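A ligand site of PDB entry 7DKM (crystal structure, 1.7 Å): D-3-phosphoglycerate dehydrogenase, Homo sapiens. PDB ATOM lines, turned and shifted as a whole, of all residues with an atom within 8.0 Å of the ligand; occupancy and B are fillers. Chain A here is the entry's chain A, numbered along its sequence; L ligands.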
ATOM      1  N   ASP A  14     -23.252 -15.789 -30.748  1.00  0.00           N
ATOM      2  CA  ASP A  14     -23.471 -14.379 -31.157  1.00  0.00           C
ATOM      3  C   ASP A  14     -22.205 -13.893 -31.878  1.00  0.00           C
ATOM      4  O   ASP A  14     -21.107 -14.199 -31.438  1.00  0.00           O
ATOM      5  CB  ASP A  14     -23.816 -13.511 -29.947  1.00  0.00           C
ATOM      6  CG  ASP A  14     -24.216 -12.081 -30.275  1.00  0.00           C
ATOM      7  OD1 ASP A  14     -23.421 -11.386 -30.931  1.00  0.00           O
ATOM      8  OD2 ASP A  14     -25.317 -11.671 -29.863  1.00  0.00           O
ATOM      9  N   PRO A  15     -22.318 -13.140 -32.996  1.00  0.00           N
ATOM     10  CA  PRO A  15     -21.159 -12.541 -33.652  1.00  0.00           C
ATOM     11  C   PRO A  15     -20.202 -11.758 -32.724  1.00  0.00           C
ATOM     12  O   PRO A  15     -19.046 -11.609 -33.078  1.00  0.00           O
ATOM     13  CB  PRO A  15     -21.795 -11.574 -34.661  1.00  0.00           C
ATOM     14  CG  PRO A  15     -23.110 -12.235 -35.017  1.00  0.00           C
ATOM     15  CD  PRO A  15     -23.566 -12.893 -33.737  1.00  0.00           C
ATOM     16  N   CYS A  16     -20.685 -11.288 -31.568  1.00  0.00           N
ATOM     17  CA  CYS A  16     -19.918 -10.469 -30.592  1.00  0.00           C
ATOM     18  C   CYS A  16     -18.752 -11.273 -29.992  1.00  0.00           C
ATOM     19  O   CYS A  16     -17.761 -10.649 -29.587  1.00  0.00           O
ATOM     20  CB  CYS A  16     -20.833  -9.961 -29.482  1.00  0.00           C
ATOM     21  SG  CYS A  16     -21.750  -8.466 -29.944  1.00  0.00           S
ATOM     22  N   CYS A  17     -18.868 -12.603 -29.920  1.00  0.00           N
ATOM     23  CA  CYS A  17     -17.796 -13.505 -29.407  1.00  0.00           C
ATOM     24  C   CYS A  17     -16.573 -13.340 -30.316  1.00  0.00           C
ATOM     25  O   CYS A  17     -15.502 -12.971 -29.798  1.00  0.00           O
ATOM     26  CB  CYS A  17     -18.247 -14.961 -29.359  1.00  0.00           C
ATOM     27  SG  CYS A  17     -17.035 -16.050 -28.569  1.00  0.00           S
ATOM     28  N   ARG A  18     -16.733 -13.560 -31.623  1.00  0.00           N
ATOM     29  CA  ARG A  18     -15.669 -13.418 -32.646  1.00  0.00           C
ATOM     30  C   ARG A  18     -15.090 -11.996 -32.596  1.00  0.00           C
ATOM     31  O   ARG A  18     -13.858 -11.857 -32.663  1.00  0.00           O
ATOM     32  CB  ARG A  18     -16.198 -13.759 -34.048  1.00  0.00           C
ATOM     33  CG  ARG A  18     -15.157 -13.580 -35.142  1.00  0.00           C
ATOM     34  CD  ARG A  18     -15.304 -14.589 -36.273  1.00  0.00           C
ATOM     35  NE  ARG A  18     -16.479 -14.305 -37.078  1.00  0.00           N
ATOM     36  CZ  ARG A  18     -16.562 -13.372 -38.030  1.00  0.00           C
ATOM     37  NH1 ARG A  18     -17.698 -13.208 -38.697  1.00  0.00           N
ATOM     38  NH2 ARG A  18     -15.523 -12.593 -38.309  1.00  0.00           N
ATOM     39  N   LYS A  19     -15.947 -10.981 -32.489  1.00  0.00           N
ATOM     40  CA  LYS A  19     -15.546  -9.546 -32.538  1.00  0.00           C
ATOM     41  C   LYS A  19     -14.591  -9.220 -31.390  1.00  0.00           C
ATOM     42  O   LYS A  19     -13.544  -8.607 -31.666  1.00  0.00           O
ATOM     43  CB  LYS A  19     -16.766  -8.611 -32.505  1.00  0.00           C
ATOM     44  CG  LYS A  19     -16.414  -7.141 -32.323  1.00  0.00           C
ATOM     45  CD  LYS A  19     -17.251  -6.182 -33.142  1.00  0.00           C
ATOM     46  CE  LYS A  19     -16.691  -4.779 -33.149  1.00  0.00           C
ATOM     47  NZ  LYS A  19     -16.848  -4.141 -34.488  1.00  0.00           N
ATOM     48  N   ILE A  20     -14.937  -9.604 -30.148  1.00  0.00           N
ATOM     49  CA  ILE A  20     -14.117  -9.344 -28.916  1.00  0.00           C
ATOM     50  C   ILE A  20     -12.748 -10.030 -29.076  1.00  0.00           C
ATOM     51  O   ILE A  20     -11.731  -9.379 -28.745  1.00  0.00           O
ATOM     52  CB  ILE A  20     -14.859  -9.828 -27.654  1.00  0.00           C
ATOM     53  CG1 ILE A  20     -16.100  -8.981 -27.359  1.00  0.00           C
ATOM     54  CG2 ILE A  20     -13.911  -9.874 -26.456  1.00  0.00           C
ATOM     55  CD1 ILE A  20     -17.130  -9.692 -26.514  1.00  0.00           C
ATOM     56  N   LEU A  21     -12.749 -11.286 -29.534  1.00  0.00           N
ATOM     57  CA  LEU A  21     -11.519 -12.092 -29.769  1.00  0.00           C
ATOM     58  C   LEU A  21     -10.616 -11.373 -30.781  1.00  0.00           C
ATOM     59  O   LEU A  21      -9.407 -11.249 -30.501  1.00  0.00           O
ATOM     60  CB  LEU A  21     -11.904 -13.488 -30.267  1.00  0.00           C
ATOM     61  CG  LEU A  21     -12.602 -14.398 -29.246  1.00  0.00           C
ATOM     62  CD1 LEU A  21     -13.037 -15.707 -29.882  1.00  0.00           C
ATOM     63  CD2 LEU A  21     -11.701 -14.666 -28.057  1.00  0.00           C
ATOM     64  N   ASP A  23     -10.792  -8.177 -31.675  1.00  0.00           N
ATOM     65  CA  ASP A  23     -10.419  -6.879 -31.033  1.00  0.00           C
ATOM     66  C   ASP A  23      -9.205  -7.097 -30.109  1.00  0.00           C
ATOM     67  O   ASP A  23      -8.415  -6.145 -29.944  1.00  0.00           O
ATOM     68  CB  ASP A  23     -11.596  -6.273 -30.262  1.00  0.00           C
ATOM     69  CG  ASP A  23     -12.655  -5.627 -31.143  1.00  0.00           C
ATOM     70  OD1 ASP A  23     -12.645  -5.863 -32.372  1.00  0.00           O
ATOM     71  OD2 ASP A  23     -13.480  -4.867 -30.593  1.00  0.00           O
ATOM     72  N   SER A 291     -26.265 -14.570 -25.295  1.00  0.00           N
ATOM     73  CA  SER A 291     -25.437 -13.424 -25.777  1.00  0.00           C
ATOM     74  C   SER A 291     -24.351 -13.073 -24.757  1.00  0.00           C
ATOM     75  O   SER A 291     -23.171 -12.969 -25.147  1.00  0.00           O
ATOM     76  CB  SER A 291     -26.307 -12.239 -26.094  1.00  0.00           C
ATOM     77  OG  SER A 291     -25.522 -11.244 -26.722  1.00  0.00           O
ATOM     78  N   GLY A 294     -21.544 -15.745 -24.469  1.00  0.00           N
ATOM     79  CA  GLY A 294     -20.692 -15.659 -25.673  1.00  0.00           C
ATOM     80  C   GLY A 294     -19.653 -14.556 -25.523  1.00  0.00           C
ATOM     81  O   GLY A 294     -18.464 -14.793 -25.851  1.00  0.00           O
ATOM     82  N   GLU A 295     -20.072 -13.404 -25.002  1.00  0.00           N
ATOM     83  CA  GLU A 295     -19.201 -12.229 -24.699  1.00  0.00           C
ATOM     84  C   GLU A 295     -18.251 -12.579 -23.548  1.00  0.00           C
ATOM     85  O   GLU A 295     -17.031 -12.346 -23.691  1.00  0.00           O
ATOM     86  CB  GLU A 295     -20.099 -11.018 -24.388  1.00  0.00           C
ATOM     87  CG  GLU A 295     -19.376  -9.831 -23.759  1.00  0.00           C
ATOM     88  CD  GLU A 295     -20.103  -8.501 -23.894  1.00  0.00           C
ATOM     89  OE1 GLU A 295     -21.238  -8.488 -24.432  1.00  0.00           O
ATOM     90  OE2 GLU A 295     -19.530  -7.480 -23.454  1.00  0.00           O
ATOM     91  N   GLU A 296     -18.782 -13.142 -22.455  1.00  0.00           N
ATOM     92  CA  GLU A 296     -18.041 -13.438 -21.205  1.00  0.00           C
ATOM     93  C   GLU A 296     -16.876 -14.388 -21.501  1.00  0.00           C
ATOM     94  O   GLU A 296     -15.809 -14.144 -20.944  1.00  0.00           O
ATOM     95  CB  GLU A 296     -18.952 -14.058 -20.149  1.00  0.00           C
ATOM     96  CG  GLU A 296     -18.283 -14.221 -18.793  1.00  0.00           C
ATOM     97  CD  GLU A 296     -19.186 -14.667 -17.675  1.00  0.00           C
ATOM     98  OE1 GLU A 296     -20.418 -14.493 -17.801  1.00  0.00           O
ATOM     99  OE2 GLU A 296     -18.673 -15.220 -16.684  1.00  0.00           O
ATOM    100  N   ALA A 298     -15.353 -14.877 -24.486  1.00  0.00           N
ATOM    101  CA  ALA A 298     -14.431 -14.133 -25.384  1.00  0.00           C
ATOM    102  C   ALA A 298     -13.527 -13.224 -24.544  1.00  0.00           C
ATOM    103  O   ALA A 298     -12.310 -13.221 -24.785  1.00  0.00           O
ATOM    104  CB  ALA A 298     -15.196 -13.350 -26.426  1.00  0.00           C
ATOM    105  N   VAL A 299     -14.117 -12.499 -23.584  1.00  0.00           N
ATOM    106  CA  VAL A 299     -13.391 -11.558 -22.673  1.00  0.00           C
ATOM    107  C   VAL A 299     -12.345 -12.347 -21.863  1.00  0.00           C
ATOM    108  O   VAL A 299     -11.212 -11.843 -21.734  1.00  0.00           O
ATOM    109  CB  VAL A 299     -14.370 -10.802 -21.748  1.00  0.00           C
ATOM    110  CG1 VAL A 299     -13.656 -10.133 -20.583  1.00  0.00           C
ATOM    111  CG2 VAL A 299     -15.173  -9.756 -22.522  1.00  0.00           C
HETATM  112  O1  LIG L   1     -18.472  -5.690 -30.030  1.00  0.00           O
HETATM  113  C1  LIG L   1     -19.135  -5.758 -29.010  1.00  0.00           C
HETATM  114  C2  LIG L   1     -18.957  -4.879 -27.794  1.00  0.00           C
HETATM  115  C3  LIG L   1     -17.567  -4.779 -27.185  1.00  0.00           C
HETATM  116  O2  LIG L   1     -17.008  -6.079 -27.039  1.00  0.00           O
HETATM  117  O3  LIG L   1     -17.733  -4.160 -25.897  1.00  0.00           O
HETATM  118  C4  LIG L   1     -18.472  -2.929 -25.937  1.00  0.00           C
HETATM  119  C5  LIG L   1     -16.639  -3.897 -28.032  1.00  0.00           C
HETATM  120  O4  LIG L   1     -16.576  -4.332 -29.392  1.00  0.00           O
HETATM  121  C6  LIG L   1     -17.143  -2.455 -28.016  1.00  0.00           C
HETATM  122  C7  LIG L   1     -16.137  -1.453 -27.409  1.00  0.00           C
HETATM  123  C8  LIG L   1     -15.158  -1.025 -28.504  1.00  0.00           C
HETATM  124  C9  LIG L   1     -15.311  -1.982 -26.222  1.00  0.00           C
HETATM  125  C10 LIG L   1     -16.864  -0.204 -26.946  1.00  0.00           C
HETATM  126  C11 LIG L   1     -18.157   0.063 -27.717  1.00  0.00           C
HETATM  127  C12 LIG L   1     -20.281  -6.698 -28.846  1.00  0.00           C
HETATM  128  C13 LIG L   1     -21.066  -7.018 -30.128  1.00  0.00           C
HETATM  129  C14 LIG L   1     -21.048  -5.958 -27.752  1.00  0.00           C
HETATM  130  C15 LIG L   1     -19.934  -5.551 -26.825  1.00  0.00           C
HETATM  131  O5  LIG L   1     -19.339  -6.683 -26.174  1.00  0.00           O
HETATM  132  C16 LIG L   1     -21.753  -4.687 -28.220  1.00  0.00           C
HETATM  133  C17 LIG L   1     -20.959  -3.385 -27.979  1.00  0.00           C
HETATM  134  C18 LIG L   1     -19.433  -3.479 -28.160  1.00  0.00           C
HETATM  135  C19 LIG L   1     -18.562  -2.446 -27.389  1.00  0.00           C
HETATM  136  C20 LIG L   1     -19.188  -1.052 -27.527  1.00  0.00           C
HETATM  137  O6  LIG L   1     -19.997  -0.771 -26.377  1.00  0.00           O
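The side-chain sulfur (SG) of Cys 16 is bonded to a carbon (C13) of the ligand, 1.6 Å away. OE2 of Glu 295 sits at hydrogen-bond distance from O5 of the ligand, at 2.8 Å. O4 of the ligand lies within hydrogen-bond range of OD2 of Asp 23 (3.4 Å).
N of Cys 16 lies within hydrogen-bond range of OD1 of Asp 14, 2.8 Å away.
Lys 19 touches the ligand (CD to O1, 3.4 Å). CG1 of Ile 20 touches O2 of the ligand, 3.1 Å away. Within 4 Å of the ligand: Cys 16, Lys 19, Ile 20, Asp 23 and Glu 295.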
